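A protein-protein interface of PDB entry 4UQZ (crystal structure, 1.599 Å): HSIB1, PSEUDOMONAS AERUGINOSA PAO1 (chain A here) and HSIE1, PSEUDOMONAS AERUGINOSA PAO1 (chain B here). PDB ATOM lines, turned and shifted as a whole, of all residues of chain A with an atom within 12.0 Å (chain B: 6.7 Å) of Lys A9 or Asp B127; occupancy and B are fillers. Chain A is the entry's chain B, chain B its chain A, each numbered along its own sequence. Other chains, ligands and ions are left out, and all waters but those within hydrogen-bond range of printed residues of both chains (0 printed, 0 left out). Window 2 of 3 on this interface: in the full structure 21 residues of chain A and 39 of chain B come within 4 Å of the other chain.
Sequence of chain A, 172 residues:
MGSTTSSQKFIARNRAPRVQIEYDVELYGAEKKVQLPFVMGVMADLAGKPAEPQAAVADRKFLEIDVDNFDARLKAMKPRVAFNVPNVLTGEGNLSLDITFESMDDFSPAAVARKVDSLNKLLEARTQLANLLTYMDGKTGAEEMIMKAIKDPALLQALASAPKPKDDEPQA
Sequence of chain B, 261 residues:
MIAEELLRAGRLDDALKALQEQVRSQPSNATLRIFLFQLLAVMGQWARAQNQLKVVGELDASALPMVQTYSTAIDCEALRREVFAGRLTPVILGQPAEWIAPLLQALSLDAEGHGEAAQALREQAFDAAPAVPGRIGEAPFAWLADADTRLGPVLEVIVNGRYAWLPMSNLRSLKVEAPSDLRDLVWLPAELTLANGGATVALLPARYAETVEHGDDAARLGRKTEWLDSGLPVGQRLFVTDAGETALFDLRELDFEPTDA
NZ of Lys A9 lies close to O of Phe B126 (3.1 Å).
The backbone carbonyl oxygen (O) of Asp B127 lies within hydrogen-bond range of the side-chain amino group (NZ) of Lys A9.
The backbone carbonyl oxygen (O) of Ala B129 sits at hydrogen-bond distance from the side-chain amino group (NZ) of Lys A9 (2.6 Å).
Among the printed residues, pairs that only touch across the chains: Gln A8 with Trp B143, Lys A9 with Trp B143, Phe A10 with Phe B126, Phe A10 with Ala B129, Phe A10 with Pro B130, Phe A10 with Trp B143, Phe A10 with Ala B145, Ile A11 with Phe B126 and Ile A11 with Trp B143.
Printed residues of chain B within 4 Å of Gln A8: Trp B143 (3.5 Å).
Of chain B, only Phe B126 (3.1 Å), Asp B127 (3.0 Å), Ala B129 (2.6 Å) and Trp B143 (3.6 Å) come within 4 Å of Lys A9.
Printed residues of chain B within 4 Å of Phe A10: Phe B126, Ala B129, Pro B130, Trp B143 and Ala B145.
Printed residues of chain B within 4 Å of Ile A11: Phe B126 (3.5 Å) and Trp B143 (3.6 Å).
No residue of chain A comes within 4 Å of Glu B123.
No residue of chain A comes within 4 Å of Gln B124.
No residue of chain A comes within 4 Å of Ala B125.
Phe B126 touches just these residues of chain A: Lys A9, Phe A10 and Ile A11.
Asp B127 touches one residue of chain A.
No residue of chain A comes within 4 Å of Ala B128.
Ala B129 touches just these residues of chain A: Lys A9 and Phe A10.
Pro B130 touches just one residue of chain A: Phe A10 (3.4 Å).
No residue of chain A comes within 4 Å of Ala B131.
Of the printed residues of chain A, Ala B145 touches Phe A10.
The nearest residue of chain A that does not touch Asp B127 is Phe A10 (5.8 Å).
Printed residues of chain B that touch a printed residue of chain A: Phe B126, Asp B127, Ala B129, Pro B130, Trp B143 and Ala B145.
Hydrophobic or aromatic side chains of chain A within 4 Å of the printed part of chain B: Phe A10 and Ile A11.
Along chain A the printed residues that touch a printed residue of chain B span positions 8 to 11.
Among the printed residues, no Asp or Glu carboxylate lies within 4 Å of a Lys or Arg side-chain nitrogen of the other chain.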
ATOM      1  N   GLN A   8      29.614 -14.402  -4.509  1.00  0.00           N
ATOM      2  CA  GLN A   8      30.507 -14.736  -5.618  1.00  0.00           C
ATOM      3  C   GLN A   8      29.843 -14.442  -6.966  1.00  0.00           C
ATOM      4  O   GLN A   8      30.520 -14.405  -8.012  1.00  0.00           O
ATOM      5  CB  GLN A   8      30.926 -16.200  -5.542  1.00  0.00           C
ATOM      6  N   LYS A   9      28.526 -14.230  -6.947  1.00  0.00           N
ATOM      7  CA  LYS A   9      27.806 -14.016  -8.210  1.00  0.00           C
ATOM      8  C   LYS A   9      28.355 -12.828  -8.975  1.00  0.00           C
ATOM      9  O   LYS A   9      28.715 -11.789  -8.406  1.00  0.00           O
ATOM     10  CB  LYS A   9      26.290 -13.864  -7.999  1.00  0.00           C
ATOM     11  CG  LYS A   9      25.791 -12.549  -7.508  1.00  0.00           C
ATOM     12  CD  LYS A   9      24.261 -12.609  -7.417  1.00  0.00           C
ATOM     13  CE  LYS A   9      23.728 -11.587  -6.449  1.00  0.00           C
ATOM     14  NZ  LYS A   9      22.352 -11.266  -6.794  1.00  0.00           N
ATOM     15  N   PHE A  10      28.492 -13.058 -10.276  1.00  0.00           N
ATOM     16  CA  PHE A  10      28.869 -12.043 -11.262  1.00  0.00           C
ATOM     17  C   PHE A  10      30.354 -11.677 -11.193  1.00  0.00           C
ATOM     18  O   PHE A  10      30.774 -10.700 -11.822  1.00  0.00           O
ATOM     19  CB  PHE A  10      28.059 -10.749 -11.096  1.00  0.00           C
ATOM     20  CG  PHE A  10      26.574 -10.940 -11.151  1.00  0.00           C
ATOM     21  CD1 PHE A  10      26.005 -11.827 -12.045  1.00  0.00           C
ATOM     22  CD2 PHE A  10      25.744 -10.228 -10.304  1.00  0.00           C
ATOM     23  CE1 PHE A  10      24.634 -11.997 -12.096  1.00  0.00           C
ATOM     24  CE2 PHE A  10      24.392 -10.393 -10.352  1.00  0.00           C
ATOM     25  CZ  PHE A  10      23.817 -11.255 -11.233  1.00  0.00           C
ATOM     26  N   ILE A  11      31.153 -12.425 -10.448  1.00  0.00           N
ATOM     27  CA  ILE A  11      32.546 -12.013 -10.259  1.00  0.00           C
ATOM     28  C   ILE A  11      33.489 -12.944 -10.992  1.00  0.00           C
ATOM     29  O   ILE A  11      33.455 -14.148 -10.755  1.00  0.00           O
ATOM     30  CB  ILE A  11      32.940 -11.984  -8.768  1.00  0.00           C
ATOM     31  CG1 ILE A  11      32.145 -10.912  -8.026  1.00  0.00           C
ATOM     32  CG2 ILE A  11      34.451 -11.752  -8.614  1.00  0.00           C
ATOM     33  CD1 ILE A  11      32.279  -9.518  -8.624  1.00  0.00           C
ATOM     34  N   ALA A  12      34.344 -12.398 -11.863  1.00  0.00           N
ATOM     35  CA  ALA A  12      35.398 -13.205 -12.455  1.00  0.00           C
ATOM     36  C   ALA A  12      36.393 -13.622 -11.384  1.00  0.00           C
ATOM     37  O   ALA A  12      36.941 -12.789 -10.667  1.00  0.00           O
ATOM     38  CB  ALA A  12      36.122 -12.448 -13.566  1.00  0.00           C
ATOM     39  N   ARG A  13      36.659 -14.913 -11.300  1.00  0.00           N
ATOM     40  CA  ARG A  13      37.531 -15.416 -10.248  1.00  0.00           C
ATOM     41  C   ARG A  13      39.014 -15.205 -10.580  1.00  0.00           C
ATOM     42  O   ARG A  13      39.859 -15.180  -9.694  1.00  0.00           O
ATOM     43  CB  ARG A  13      37.246 -16.902  -9.993  1.00  0.00           C
ATOM     44  CG  ARG A  13      35.816 -17.187  -9.525  1.00  0.00           C
ATOM     45  CD  ARG A  13      35.498 -18.682  -9.497  1.00  0.00           C
ATOM     46  NE  ARG A  13      35.868 -19.356 -10.743  1.00  0.00           N
ATOM     47  CZ  ARG A  13      35.070 -19.478 -11.803  1.00  0.00           C
ATOM     48  NH1 ARG A  13      33.840 -18.969 -11.781  1.00  0.00           N
ATOM     49  NH2 ARG A  13      35.503 -20.114 -12.886  1.00  0.00           N
ATOM     50  N   ASN A  14      39.309 -15.030 -11.854  1.00  0.00           N
ATOM     51  CA  ASN A  14      40.679 -14.942 -12.335  1.00  0.00           C
ATOM     52  C   ASN A  14      40.864 -13.658 -13.153  1.00  0.00           C
ATOM     53  O   ASN A  14      40.069 -13.405 -14.028  1.00  0.00           O
ATOM     54  CB  ASN A  14      40.992 -16.206 -13.168  1.00  0.00           C
ATOM     55  CG  ASN A  14      42.166 -16.038 -14.108  1.00  0.00           C
ATOM     56  OD1 ASN A  14      43.097 -15.289 -13.836  1.00  0.00           O
ATOM     57  ND2 ASN A  14      42.143 -16.780 -15.218  1.00  0.00           N
ATOM     58  N   ARG A  15      41.878 -12.848 -12.843  1.00  0.00           N
ATOM     59  CA  ARG A  15      42.176 -11.673 -13.672  1.00  0.00           C
ATOM     60  C   ARG A  15      43.548 -11.758 -14.336  1.00  0.00           C
ATOM     61  O   ARG A  15      44.172 -10.733 -14.637  1.00  0.00           O
ATOM     62  CB  ARG A  15      42.060 -10.389 -12.848  1.00  0.00           C
ATOM     63  CG  ARG A  15      40.644 -10.111 -12.374  1.00  0.00           C
ATOM     64  CD  ARG A  15      40.615  -8.853 -11.530  1.00  0.00           C
ATOM     65  NE  ARG A  15      39.409  -8.061 -11.740  1.00  0.00           N
ATOM     66  CZ  ARG A  15      39.368  -6.740 -11.584  1.00  0.00           C
ATOM     67  NH1 ARG A  15      40.468  -6.091 -11.221  1.00  0.00           N
ATOM     68  NH2 ARG A  15      38.238  -6.068 -11.780  1.00  0.00           N
ATOM     69  N   TRP B  99      18.777  -1.339  -9.652  1.00  0.00           N
ATOM     70  CA  TRP B  99      20.160  -1.527  -9.256  1.00  0.00           C
ATOM     71  C   TRP B  99      21.151  -0.926 -10.258  1.00  0.00           C
ATOM     72  O   TRP B  99      22.351  -0.930 -10.031  1.00  0.00           O
ATOM     73  CB  TRP B  99      20.458  -3.026  -9.070  1.00  0.00           C
ATOM     74  CG  TRP B  99      19.987  -3.887 -10.181  1.00  0.00           C
ATOM     75  CD1 TRP B  99      18.799  -4.543 -10.269  1.00  0.00           C
ATOM     76  CD2 TRP B  99      20.701  -4.184 -11.380  1.00  0.00           C
ATOM     77  NE1 TRP B  99      18.729  -5.233 -11.443  1.00  0.00           N
ATOM     78  CE2 TRP B  99      19.888  -5.044 -12.143  1.00  0.00           C
ATOM     79  CE3 TRP B  99      21.971  -3.851 -11.856  1.00  0.00           C
ATOM     80  CZ2 TRP B  99      20.276  -5.523 -13.400  1.00  0.00           C
ATOM     81  CZ3 TRP B  99      22.371  -4.332 -13.095  1.00  0.00           C
ATOM     82  CH2 TRP B  99      21.527  -5.176 -13.854  1.00  0.00           C
ATOM     83  N   ARG B 122      28.706  -0.729  -5.803  1.00  0.00           N
ATOM     84  CA  ARG B 122      28.727  -1.855  -6.752  1.00  0.00           C
ATOM     85  C   ARG B 122      28.385  -3.154  -6.059  1.00  0.00           C
ATOM     86  O   ARG B 122      27.695  -4.008  -6.641  1.00  0.00           O
ATOM     87  CB  ARG B 122      30.086  -1.981  -7.455  1.00  0.00           C
ATOM     88  CG  ARG B 122      30.296  -0.873  -8.406  1.00  0.00           C
ATOM     89  CD  ARG B 122      31.503  -1.133  -9.276  1.00  0.00           C
ATOM     90  NE  ARG B 122      31.612  -0.001 -10.179  1.00  0.00           N
ATOM     91  CZ  ARG B 122      32.533   0.957 -10.092  1.00  0.00           C
ATOM     92  NH1 ARG B 122      33.490   0.890  -9.174  1.00  0.00           N
ATOM     93  NH2 ARG B 122      32.497   1.978 -10.945  1.00  0.00           N
ATOM     94  N   GLU B 123      28.820  -3.296  -4.810  1.00  0.00           N
ATOM     95  CA  GLU B 123      28.506  -4.494  -4.077  1.00  0.00           C
ATOM     96  C   GLU B 123      27.003  -4.548  -3.865  1.00  0.00           C
ATOM     97  O   GLU B 123      26.392  -5.588  -4.077  1.00  0.00           O
ATOM     98  CB  GLU B 123      29.265  -4.552  -2.757  1.00  0.00           C
ATOM     99  CG  GLU B 123      30.750  -4.844  -2.935  1.00  0.00           C
ATOM    100  CD  GLU B 123      31.553  -4.733  -1.634  1.00  0.00           C
ATOM    101  OE1 GLU B 123      30.940  -4.584  -0.548  1.00  0.00           O
ATOM    102  OE2 GLU B 123      32.806  -4.798  -1.706  1.00  0.00           O
ATOM    103  N   GLN B 124      26.410  -3.406  -3.530  1.00  0.00           N
ATOM    104  CA  GLN B 124      24.969  -3.364  -3.355  1.00  0.00           C
ATOM    105  C   GLN B 124      24.214  -3.619  -4.668  1.00  0.00           C
ATOM    106  O   GLN B 124      23.181  -4.309  -4.681  1.00  0.00           O
ATOM    107  CB  GLN B 124      24.538  -2.025  -2.725  1.00  0.00           C
ATOM    108  CG  GLN B 124      25.132  -1.798  -1.352  1.00  0.00           C
ATOM    109  CD  GLN B 124      24.997  -0.369  -0.919  1.00  0.00           C
ATOM    110  OE1 GLN B 124      24.303   0.414  -1.575  1.00  0.00           O
ATOM    111  NE2 GLN B 124      25.652  -0.013   0.185  1.00  0.00           N
ATOM    112  N   ALA B 125      24.741  -3.081  -5.763  1.00  0.00           N
ATOM    113  CA  ALA B 125      24.115  -3.293  -7.053  1.00  0.00           C
ATOM    114  C   ALA B 125      24.145  -4.757  -7.442  1.00  0.00           C
ATOM    115  O   ALA B 125      23.152  -5.327  -7.890  1.00  0.00           O
ATOM    116  CB  ALA B 125      24.822  -2.464  -8.123  1.00  0.00           C
ATOM    117  N   PHE B 126      25.320  -5.354  -7.299  1.00  0.00           N
ATOM    118  CA  PHE B 126      25.480  -6.781  -7.593  1.00  0.00           C
ATOM    119  C   PHE B 126      24.570  -7.663  -6.736  1.00  0.00           C
ATOM    120  O   PHE B 126      23.987  -8.636  -7.218  1.00  0.00           O
ATOM    121  CB  PHE B 126      26.942  -7.209  -7.400  1.00  0.00           C
ATOM    122  CG  PHE B 126      27.843  -6.909  -8.593  1.00  0.00           C
ATOM    123  CD1 PHE B 126      27.712  -5.760  -9.356  1.00  0.00           C
ATOM    124  CD2 PHE B 126      28.810  -7.812  -8.924  1.00  0.00           C
ATOM    125  CE1 PHE B 126      28.573  -5.517 -10.447  1.00  0.00           C
ATOM    126  CE2 PHE B 126      29.653  -7.576 -10.010  1.00  0.00           C
ATOM    127  CZ  PHE B 126      29.547  -6.452 -10.724  1.00  0.00           C
ATOM    128  N   ASP B 127      24.473  -7.345  -5.440  1.00  0.00           N
ATOM    129  CA  ASP B 127      23.582  -8.066  -4.538  1.00  0.00           C
ATOM    130  C   ASP B 127      22.148  -8.028  -5.037  1.00  0.00           C
ATOM    131  O   ASP B 127      21.462  -9.042  -5.043  1.00  0.00           O
ATOM    132  CB  ASP B 127      23.665  -7.466  -3.141  1.00  0.00           C
ATOM    133  CG  ASP B 127      24.733  -8.109  -2.292  1.00  0.00           C
ATOM    134  OD1 ASP B 127      24.771  -9.360  -2.225  1.00  0.00           O
ATOM    135  OD2 ASP B 127      25.529  -7.366  -1.675  1.00  0.00           O
ATOM    136  N   ALA B 128      21.721  -6.854  -5.482  1.00  0.00           N
ATOM    137  CA  ALA B 128      20.349  -6.649  -5.900  1.00  0.00           C
ATOM    138  C   ALA B 128      20.051  -7.246  -7.280  1.00  0.00           C
ATOM    139  O   ALA B 128      18.943  -7.721  -7.520  1.00  0.00           O
ATOM    140  CB  ALA B 128      20.017  -5.139  -5.890  1.00  0.00           C
ATOM    141  N   ALA B 129      21.034  -7.237  -8.181  1.00  0.00           N
ATOM    142  CA  ALA B 129      20.827  -7.744  -9.542  1.00  0.00           C
ATOM    143  C   ALA B 129      20.549  -9.252  -9.476  1.00  0.00           C
ATOM    144  O   ALA B 129      21.264  -9.976  -8.795  1.00  0.00           O
ATOM    145  CB  ALA B 129      22.030  -7.460 -10.390  1.00  0.00           C
ATOM    146  N   PRO B 130      19.531  -9.731 -10.204  1.00  0.00           N
ATOM    147  CA  PRO B 130      19.110 -11.139 -10.100  1.00  0.00           C
ATOM    148  C   PRO B 130      20.060 -12.112 -10.827  1.00  0.00           C
ATOM    149  O   PRO B 130      20.501 -11.845 -11.935  1.00  0.00           O
ATOM    150  CB  PRO B 130      17.728 -11.130 -10.753  1.00  0.00           C
ATOM    151  CG  PRO B 130      17.807  -9.999 -11.772  1.00  0.00           C
ATOM    152  CD  PRO B 130      18.711  -8.965 -11.169  1.00  0.00           C
ATOM    153  N   ALA B 131      20.389 -13.221 -10.184  1.00  0.00           N
ATOM    154  CA  ALA B 131      21.082 -14.285 -10.899  1.00  0.00           C
ATOM    155  C   ALA B 131      20.018 -14.957 -11.758  1.00  0.00           C
ATOM    156  O   ALA B 131      19.012 -15.473 -11.230  1.00  0.00           O
ATOM    157  CB  ALA B 131      21.753 -15.285  -9.930  1.00  0.00           C
ATOM    158  N   TRP B 143      24.567 -18.139 -13.378  1.00  0.00           N
ATOM    159  CA  TRP B 143      24.564 -16.698 -13.550  1.00  0.00           C
ATOM    160  C   TRP B 143      25.597 -16.327 -14.568  1.00  0.00           C
ATOM    161  O   TRP B 143      26.494 -17.109 -14.854  1.00  0.00           O
ATOM    162  CB  TRP B 143      24.833 -15.940 -12.249  1.00  0.00           C
ATOM    163  CG  TRP B 143      26.052 -16.358 -11.482  1.00  0.00           C
ATOM    164  CD1 TRP B 143      26.065 -17.088 -10.342  1.00  0.00           C
ATOM    165  CD2 TRP B 143      27.410 -15.990 -11.738  1.00  0.00           C
ATOM    166  NE1 TRP B 143      27.347 -17.248  -9.882  1.00  0.00           N
ATOM    167  CE2 TRP B 143      28.199 -16.581 -10.720  1.00  0.00           C
ATOM    168  CE3 TRP B 143      28.046 -15.233 -12.744  1.00  0.00           C
ATOM    169  CZ2 TRP B 143      29.594 -16.451 -10.670  1.00  0.00           C
ATOM    170  CZ3 TRP B 143      29.443 -15.113 -12.701  1.00  0.00           C
ATOM    171  CH2 TRP B 143      30.200 -15.732 -11.663  1.00  0.00           C
ATOM    172  N   ALA B 145      27.781 -12.666 -16.199  1.00  0.00           N
ATOM    173  CA  ALA B 145      28.027 -11.224 -16.152  1.00  0.00           C
ATOM    174  C   ALA B 145      29.212 -10.883 -17.022  1.00  0.00           C
ATOM    175  O   ALA B 145      29.979 -11.760 -17.420  1.00  0.00           O
ATOM    176  CB  ALA B 145      28.294 -10.771 -14.720  1.00  0.00           C
